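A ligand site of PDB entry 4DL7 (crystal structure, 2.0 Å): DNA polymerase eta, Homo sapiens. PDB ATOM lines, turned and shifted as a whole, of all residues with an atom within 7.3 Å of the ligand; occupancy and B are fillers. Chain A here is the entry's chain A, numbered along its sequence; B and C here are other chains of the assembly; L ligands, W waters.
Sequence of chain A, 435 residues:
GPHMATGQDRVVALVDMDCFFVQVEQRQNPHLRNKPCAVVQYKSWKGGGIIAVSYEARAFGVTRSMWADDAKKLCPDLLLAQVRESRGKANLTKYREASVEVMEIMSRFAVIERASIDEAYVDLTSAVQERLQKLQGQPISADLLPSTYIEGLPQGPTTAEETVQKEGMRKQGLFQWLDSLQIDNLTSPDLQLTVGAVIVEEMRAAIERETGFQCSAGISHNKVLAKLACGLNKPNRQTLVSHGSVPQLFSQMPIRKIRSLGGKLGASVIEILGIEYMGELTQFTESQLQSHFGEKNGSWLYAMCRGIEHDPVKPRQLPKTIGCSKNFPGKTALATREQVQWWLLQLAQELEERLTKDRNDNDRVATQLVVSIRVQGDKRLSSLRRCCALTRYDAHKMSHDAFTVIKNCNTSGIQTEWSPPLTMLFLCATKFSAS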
ATOM      1  N   VAL A 224      -1.302  -1.572  23.916  1.00  0.00           N
ATOM      2  CA  VAL A 224      -0.041  -2.315  23.941  1.00  0.00           C
ATOM      3  C   VAL A 224       1.113  -1.534  23.305  1.00  0.00           C
ATOM      4  O   VAL A 224       2.190  -1.443  23.886  1.00  0.00           O
ATOM      5  CB  VAL A 224      -0.168  -3.687  23.256  1.00  0.00           C
ATOM      6  CG1 VAL A 224       1.182  -4.392  23.206  1.00  0.00           C
ATOM      7  CG2 VAL A 224      -1.184  -4.552  24.001  1.00  0.00           C
ATOM      8  N   ARG A 259       3.479  -6.273  26.588  1.00  0.00           N
ATOM      9  CA  ARG A 259       2.715  -6.438  27.789  1.00  0.00           C
ATOM     10  C   ARG A 259       1.878  -7.709  27.779  1.00  0.00           C
ATOM     11  O   ARG A 259       1.208  -7.968  26.811  1.00  0.00           O
ATOM     12  CB  ARG A 259       1.808  -5.248  27.953  1.00  0.00           C
ATOM     13  CG  ARG A 259       1.512  -5.014  29.380  1.00  0.00           C
ATOM     14  CD  ARG A 259       0.122  -5.398  29.688  1.00  0.00           C
ATOM     15  NE  ARG A 259      -0.722  -4.349  29.216  1.00  0.00           N
ATOM     16  CZ  ARG A 259      -1.735  -4.517  28.397  1.00  0.00           C
ATOM     17  NH1 ARG A 259      -2.435  -3.444  28.040  1.00  0.00           N
ATOM     18  NH2 ARG A 259      -2.066  -5.713  27.970  1.00  0.00           N
ATOM     19  N   SER A 260       1.946  -8.458  28.866  1.00  0.00           N
ATOM     20  CA  SER A 260       1.269  -9.741  29.059  1.00  0.00           C
ATOM     21  C   SER A 260       2.092 -10.922  28.548  1.00  0.00           C
ATOM     22  O   SER A 260       1.748 -12.072  28.781  1.00  0.00           O
ATOM     23  CB  SER A 260      -0.126  -9.731  28.423  1.00  0.00           C
ATOM     24  OG  SER A 260      -0.101 -10.120  27.075  1.00  0.00           O
ATOM     25  N   LEU A 261       3.198 -10.623  27.871  1.00  0.00           N
ATOM     26  CA  LEU A 261       4.091 -11.646  27.363  1.00  0.00           C
ATOM     27  C   LEU A 261       5.349 -11.827  28.201  1.00  0.00           C
ATOM     28  O   LEU A 261       6.245 -12.567  27.833  1.00  0.00           O
ATOM     29  CB  LEU A 261       4.433 -11.388  25.893  1.00  0.00           C
ATOM     30  CG  LEU A 261       3.248 -11.438  24.934  1.00  0.00           C
ATOM     31  CD1 LEU A 261       3.684 -11.559  23.491  1.00  0.00           C
ATOM     32  CD2 LEU A 261       2.262 -12.539  25.303  1.00  0.00           C
ATOM     33  N   LEU A 265       3.445 -17.457  29.470  1.00  0.00           N
ATOM     34  CA  LEU A 265       2.950 -17.522  28.094  1.00  0.00           C
ATOM     35  C   LEU A 265       4.036 -17.088  27.113  1.00  0.00           C
ATOM     36  O   LEU A 265       4.285 -17.756  26.121  1.00  0.00           O
ATOM     37  CB  LEU A 265       1.715 -16.645  27.921  1.00  0.00           C
ATOM     38  CG  LEU A 265       1.234 -16.514  26.468  1.00  0.00           C
ATOM     39  CD1 LEU A 265       0.865 -17.882  25.901  1.00  0.00           C
ATOM     40  CD2 LEU A 265       0.064 -15.549  26.354  1.00  0.00           C
ATOM     41  N   PHE A 293      -1.606 -21.970  21.739  1.00  0.00           N
ATOM     42  CA  PHE A 293      -1.794 -21.077  22.878  1.00  0.00           C
ATOM     43  C   PHE A 293      -3.256 -20.794  23.214  1.00  0.00           C
ATOM     44  O   PHE A 293      -3.544 -19.970  24.083  1.00  0.00           O
ATOM     45  CB  PHE A 293      -1.041 -19.772  22.650  1.00  0.00           C
ATOM     46  CG  PHE A 293       0.363 -19.970  22.146  1.00  0.00           C
ATOM     47  CD1 PHE A 293       1.329 -20.539  22.965  1.00  0.00           C
ATOM     48  CD2 PHE A 293       0.713 -19.589  20.862  1.00  0.00           C
ATOM     49  CE1 PHE A 293       2.614 -20.727  22.506  1.00  0.00           C
ATOM     50  CE2 PHE A 293       1.999 -19.770  20.397  1.00  0.00           C
ATOM     51  CZ  PHE A 293       2.954 -20.343  21.222  1.00  0.00           C
ATOM     52  N   GLU A 295      -7.552 -20.335  21.771  1.00  0.00           N
ATOM     53  CA  GLU A 295      -8.314 -19.505  20.845  1.00  0.00           C
ATOM     54  C   GLU A 295      -8.093 -18.009  21.067  1.00  0.00           C
ATOM     55  O   GLU A 295      -7.776 -17.270  20.131  1.00  0.00           O
ATOM     56  CB  GLU A 295      -9.802 -19.835  20.954  1.00  0.00           C
ATOM     57  CG  GLU A 295     -10.681 -19.126  19.930  1.00  0.00           C
ATOM     58  CD  GLU A 295     -12.156 -19.345  20.194  1.00  0.00           C
ATOM     59  OE1 GLU A 295     -12.735 -18.562  20.969  1.00  0.00           O
ATOM     60  OE2 GLU A 295     -12.733 -20.302  19.627  1.00  0.00           O
ATOM     61  N   LYS A 296      -8.318 -17.535  22.293  1.00  0.00           N
ATOM     62  CA  LYS A 296      -8.133 -16.124  22.640  1.00  0.00           C
ATOM     63  C   LYS A 296      -6.708 -15.589  22.542  1.00  0.00           C
ATOM     64  O   LYS A 296      -6.465 -14.675  21.769  1.00  0.00           O
ATOM     65  CB  LYS A 296      -8.698 -15.848  24.032  1.00  0.00           C
ATOM     66  CG  LYS A 296      -8.247 -14.525  24.629  1.00  0.00           C
ATOM     67  CD  LYS A 296      -9.267 -13.934  25.601  1.00  0.00           C
ATOM     68  CE  LYS A 296     -10.182 -14.989  26.187  1.00  0.00           C
ATOM     69  NZ  LYS A 296     -11.519 -15.000  25.541  1.00  0.00           N
ATOM     70  N   ASN A 297      -5.757 -16.373  23.029  1.00  0.00           N
ATOM     71  CA  ASN A 297      -4.349 -15.994  22.927  1.00  0.00           C
ATOM     72  C   ASN A 297      -3.821 -15.993  21.496  1.00  0.00           C
ATOM     73  O   ASN A 297      -3.100 -15.086  21.095  1.00  0.00           O
ATOM     74  CB  ASN A 297      -3.471 -16.893  23.815  1.00  0.00           C
ATOM     75  CG  ASN A 297      -3.598 -16.566  25.285  1.00  0.00           C
ATOM     76  OD1 ASN A 297      -4.017 -15.478  25.660  1.00  0.00           O
ATOM     77  ND2 ASN A 297      -3.220 -17.520  26.138  1.00  0.00           N
ATOM     78  N   GLY A 298      -4.199 -17.030  20.739  1.00  0.00           N
ATOM     79  CA  GLY A 298      -3.760 -17.151  19.360  1.00  0.00           C
ATOM     80  C   GLY A 298      -4.192 -15.992  18.490  1.00  0.00           C
ATOM     81  O   GLY A 298      -3.384 -15.426  17.741  1.00  0.00           O
ATOM     82  N   SER A 299      -5.471 -15.630  18.570  1.00  0.00           N
ATOM     83  CA  SER A 299      -6.001 -14.511  17.817  1.00  0.00           C
ATOM     84  C   SER A 299      -5.325 -13.210  18.238  1.00  0.00           C
ATOM     85  O   SER A 299      -4.999 -12.367  17.399  1.00  0.00           O
ATOM     86  CB  SER A 299      -7.511 -14.397  17.999  1.00  0.00           C
ATOM     87  OG  SER A 299      -8.185 -15.433  17.310  1.00  0.00           O
ATOM     88  N   TRP A 300      -5.118 -13.050  19.542  1.00  0.00           N
ATOM     89  CA  TRP A 300      -4.482 -11.846  20.073  1.00  0.00           C
ATOM     90  C   TRP A 300      -3.061 -11.714  19.530  1.00  0.00           C
ATOM     91  O   TRP A 300      -2.639 -10.635  19.102  1.00  0.00           O
ATOM     92  CB  TRP A 300      -4.468 -11.876  21.593  1.00  0.00           C
ATOM     93  CG  TRP A 300      -3.948 -10.617  22.211  1.00  0.00           C
ATOM     94  CD1 TRP A 300      -4.646  -9.465  22.447  1.00  0.00           C
ATOM     95  CD2 TRP A 300      -2.612 -10.371  22.664  1.00  0.00           C
ATOM     96  NE1 TRP A 300      -3.825  -8.525  23.023  1.00  0.00           N
ATOM     97  CE2 TRP A 300      -2.568  -9.053  23.166  1.00  0.00           C
ATOM     98  CE3 TRP A 300      -1.438 -11.137  22.702  1.00  0.00           C
ATOM     99  CZ2 TRP A 300      -1.417  -8.484  23.694  1.00  0.00           C
ATOM    100  CZ3 TRP A 300      -0.290 -10.574  23.222  1.00  0.00           C
ATOM    101  CH2 TRP A 300      -0.289  -9.266  23.717  1.00  0.00           C
ATOM    102  N   LEU A 301      -2.320 -12.818  19.555  1.00  0.00           N
ATOM    103  CA  LEU A 301      -0.941 -12.830  19.080  1.00  0.00           C
ATOM    104  C   LEU A 301      -0.851 -12.543  17.582  1.00  0.00           C
ATOM    105  O   LEU A 301       0.023 -11.803  17.144  1.00  0.00           O
ATOM    106  CB  LEU A 301      -0.281 -14.181  19.391  1.00  0.00           C
ATOM    107  CG  LEU A 301       0.080 -14.431  20.860  1.00  0.00           C
ATOM    108  CD1 LEU A 301       0.315 -15.911  21.111  1.00  0.00           C
ATOM    109  CD2 LEU A 301       1.288 -13.605  21.268  1.00  0.00           C
ATOM    110  N   GLU A 309      -4.300  -4.230  18.005  1.00  0.00           N
ATOM    111  CA  GLU A 309      -4.875  -4.606  19.286  1.00  0.00           C
ATOM    112  C   GLU A 309      -6.157  -3.819  19.501  1.00  0.00           C
ATOM    113  O   GLU A 309      -6.202  -2.612  19.236  1.00  0.00           O
ATOM    114  CB  GLU A 309      -3.886  -4.336  20.415  1.00  0.00           C
ATOM    115  CG  GLU A 309      -4.034  -5.269  21.604  1.00  0.00           C
ATOM    116  CD  GLU A 309      -4.314  -4.524  22.891  1.00  0.00           C
ATOM    117  OE1 GLU A 309      -4.811  -5.162  23.855  1.00  0.00           O
ATOM    118  OE2 GLU A 309      -4.033  -3.305  22.965  1.00  0.00           O
ATOM    119  N   ASP A 311      -8.203  -3.925  22.476  1.00  0.00           N
ATOM    120  CA  ASP A 311      -8.595  -3.699  23.868  1.00  0.00           C
ATOM    121  C   ASP A 311      -8.936  -2.223  24.080  1.00  0.00           C
ATOM    122  O   ASP A 311      -8.081  -1.353  23.907  1.00  0.00           O
ATOM    123  CB  ASP A 311      -7.510  -4.145  24.834  1.00  0.00           C
ATOM    124  CG  ASP A 311      -7.990  -4.160  26.277  1.00  0.00           C
ATOM    125  OD1 ASP A 311      -7.224  -3.748  27.169  1.00  0.00           O
ATOM    126  OD2 ASP A 311      -9.146  -4.587  26.512  1.00  0.00           O
ATOM    127  P    DC B   9      -9.771  -4.745  34.255  1.00  0.00           P
ATOM    128  OP1  DC B   9      -9.964  -3.902  33.060  1.00  0.00           O
ATOM    129  OP2  DC B   9     -10.817  -4.815  35.293  1.00  0.00           O
ATOM    130  O5'  DC B   9      -9.466  -6.242  33.785  1.00  0.00           O
ATOM    131  C5'  DC B   9      -8.279  -6.528  33.052  1.00  0.00           C
ATOM    132  C4'  DC B   9      -8.093  -8.016  32.898  1.00  0.00           C
ATOM    133  O4'  DC B   9      -7.637  -8.594  34.149  1.00  0.00           O
ATOM    134  C3'  DC B   9      -9.349  -8.788  32.511  1.00  0.00           C
ATOM    135  O3'  DC B   9      -9.053  -9.623  31.405  1.00  0.00           O
ATOM    136  C2'  DC B   9      -9.716  -9.571  33.762  1.00  0.00           C
ATOM    137  C1'  DC B   9      -8.351  -9.786  34.396  1.00  0.00           C
ATOM    138  N1   DC B   9      -8.395 -10.001  35.867  1.00  0.00           N
ATOM    139  C2   DC B   9      -7.698 -11.081  36.422  1.00  0.00           C
ATOM    140  O2   DC B   9      -7.058 -11.830  35.672  1.00  0.00           O
ATOM    141  N3   DC B   9      -7.751 -11.271  37.761  1.00  0.00           N
ATOM    142  C4   DC B   9      -8.454 -10.442  38.529  1.00  0.00           C
ATOM    143  N4   DC B   9      -8.475 -10.667  39.848  1.00  0.00           N
ATOM    144  C5   DC B   9      -9.174  -9.335  37.984  1.00  0.00           C
ATOM    145  C6   DC B   9      -9.115  -9.163  36.657  1.00  0.00           C
ATOM    146  P    DA B  10     -10.206 -10.464  30.688  1.00  0.00           P
ATOM    147  OP1  DA B  10     -10.234 -10.082  29.260  1.00  0.00           O
ATOM    148  OP2  DA B  10     -11.433 -10.353  31.500  1.00  0.00           O
ATOM    149  O5'  DA B  10      -9.694 -11.969  30.805  1.00  0.00           O
ATOM    150  C5'  DA B  10      -8.322 -12.265  30.590  1.00  0.00           C
ATOM    151  C4'  DA B  10      -8.068 -13.745  30.798  1.00  0.00           C
ATOM    152  O4'  DA B  10      -7.925 -14.030  32.215  1.00  0.00           O
ATOM    153  C3'  DA B  10      -9.176 -14.651  30.301  1.00  0.00           C
ATOM    154  O3'  DA B  10      -8.613 -15.839  29.777  1.00  0.00           O
ATOM    155  C2'  DA B  10     -10.019 -14.898  31.557  1.00  0.00           C
ATOM    156  C1'  DA B  10      -8.940 -14.924  32.637  1.00  0.00           C
ATOM    157  N9   DA B  10      -9.409 -14.494  33.953  1.00  0.00           N
ATOM    158  C8   DA B  10     -10.181 -13.403  34.240  1.00  0.00           C
ATOM    159  N7   DA B  10     -10.433 -13.258  35.520  1.00  0.00           N
ATOM    160  C5   DA B  10      -9.785 -14.329  36.106  1.00  0.00           C
ATOM    161  C6   DA B  10      -9.666 -14.746  37.451  1.00  0.00           C
ATOM    162  N6   DA B  10     -10.231 -14.113  38.479  1.00  0.00           N
ATOM    163  N1   DA B  10      -8.941 -15.864  37.696  1.00  0.00           N
ATOM    164  C2   DA B  10      -8.377 -16.503  36.660  1.00  0.00           C
ATOM    165  N3   DA B  10      -8.420 -16.206  35.364  1.00  0.00           N
ATOM    166  C4   DA B  10      -9.147 -15.099  35.153  1.00  0.00           C
ATOM    167  P    DC B  11      -9.554 -16.959  29.111  1.00  0.00           P
ATOM    168  OP1  DC B  11      -8.880 -17.451  27.898  1.00  0.00           O
ATOM    169  OP2  DC B  11     -10.927 -16.409  29.029  1.00  0.00           O
ATOM    170  O5'  DC B  11      -9.576 -18.118  30.200  1.00  0.00           O
ATOM    171  C5'  DC B  11      -8.341 -18.556  30.767  1.00  0.00           C
ATOM    172  C4'  DC B  11      -8.587 -19.611  31.815  1.00  0.00           C
ATOM    173  O4'  DC B  11      -9.003 -18.995  33.052  1.00  0.00           O
ATOM    174  C3'  DC B  11      -9.657 -20.639  31.466  1.00  0.00           C
ATOM    175  O3'  DC B  11      -9.126 -21.922  31.716  1.00  0.00           O
ATOM    176  C2'  DC B  11     -10.829 -20.282  32.385  1.00  0.00           C
ATOM    177  C1'  DC B  11     -10.107 -19.683  33.591  1.00  0.00           C
ATOM    178  N1   DC B  11     -10.893 -18.689  34.380  1.00  0.00           N
ATOM    179  C2   DC B  11     -10.951 -18.824  35.767  1.00  0.00           C
ATOM    180  O2   DC B  11     -10.367 -19.772  36.311  1.00  0.00           O
ATOM    181  N3   DC B  11     -11.657 -17.916  36.487  1.00  0.00           N
ATOM    182  C4   DC B  11     -12.269 -16.902  35.873  1.00  0.00           C
ATOM    183  N4   DC B  11     -12.942 -16.035  36.631  1.00  0.00           N
ATOM    184  C5   DC B  11     -12.217 -16.747  34.459  1.00  0.00           C
ATOM    185  C6   DC B  11     -11.521 -17.655  33.754  1.00  0.00           C
ATOM    186  P    DC C   7       1.979 -15.471  32.832  1.00  0.00           P
ATOM    187  OP1  DC C   7       2.008 -15.739  31.376  1.00  0.00           O
ATOM    188  OP2  DC C   7       3.042 -16.035  33.713  1.00  0.00           O
ATOM    189  O5'  DC C   7       1.953 -13.892  33.059  1.00  0.00           O
ATOM    190  C5'  DC C   7       0.941 -13.119  32.414  1.00  0.00           C
ATOM    191  C4'  DC C   7       0.839 -11.753  33.066  1.00  0.00           C
ATOM    192  O4'  DC C   7       0.203 -11.872  34.356  1.00  0.00           O
ATOM    193  C3'  DC C   7       2.173 -11.060  33.330  1.00  0.00           C
ATOM    194  O3'  DC C   7       2.415 -10.109  32.298  1.00  0.00           O
ATOM    195  C2'  DC C   7       1.998 -10.409  34.703  1.00  0.00           C
ATOM    196  C1'  DC C   7       0.548 -10.713  35.078  1.00  0.00           C
ATOM    197  N1   DC C   7       0.329 -10.970  36.532  1.00  0.00           N
ATOM    198  C2   DC C   7      -0.619 -10.204  37.224  1.00  0.00           C
ATOM    199  O2   DC C   7      -1.232  -9.321  36.609  1.00  0.00           O
ATOM    200  N3   DC C   7      -0.819 -10.443  38.545  1.00  0.00           N
ATOM    201  C4   DC C   7      -0.142 -11.401  39.165  1.00  0.00           C
ATOM    202  N4   DC C   7      -0.382 -11.592  40.470  1.00  0.00           N
ATOM    203  C5   DC C   7       0.821 -12.193  38.476  1.00  0.00           C
ATOM    204  C6   DC C   7       1.023 -11.950  37.178  1.00  0.00           C
HETATM  205  N1  LIG L   1      -3.472 -10.740  27.224  1.00  0.00           N
HETATM  206  C1  LIG L   1      -4.505  -9.895  27.158  1.00  0.00           C
HETATM  207  N2  LIG L   1      -5.614  -9.965  26.402  1.00  0.00           N
HETATM  208  C2  LIG L   1      -5.605 -11.063  25.654  1.00  0.00           C
HETATM  209  C3  LIG L   1      -4.601 -12.010  25.652  1.00  0.00           C
HETATM  210  C4  LIG L   1      -3.484 -11.839  26.469  1.00  0.00           C
HETATM  211  N3  LIG L   1      -2.482 -12.716  26.503  1.00  0.00           N
HETATM  212  N4  LIG L   1      -4.879 -12.999  24.771  1.00  0.00           N
HETATM  213  C5  LIG L   1      -6.025 -12.672  24.283  1.00  0.00           C
HETATM  214  N5  LIG L   1      -6.549 -11.524  24.751  1.00  0.00           N
HETATM  215  C6  LIG L   1      -7.813 -10.974  24.297  1.00  0.00           C
HETATM  216  O   HOH W   1      -0.780 -13.124  29.197  1.00  0.00           O
HETATM  217  O   HOH W   2      -8.366 -12.531  21.403  1.00  0.00           O
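The side-chain hydroxyl of Ser 260 is in hydrogen-bond range of a nitrogen (N1) of the ligand.
N4 of the ligand lies close to OD1 of Asn 297 (2.8 Å).
OP2 of DC 11 of chain B lies within salt-bridge range of the side-chain amino group (NZ) of Lys 296 (3.8 Å).
ND2 of Asn 297 sits close to O of Phe 293, 3.2 Å away.
N of Leu 265 sits at hydrogen-bond distance from OP1 of DC 7 of chain C (2.9 Å).
Merely in contact with the ligand: Lys 296 (2.9 Å), Trp 300 (3.2 Å) and Leu 265 (3.8 Å).
Hydrophobic or aromatic side chains within 4 Å of the ligand: Leu 265 and Trp 300.
Water W1 bridges the backbone carbonyl oxygen of Ser 260 and a nitrogen (N3) of the ligand.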
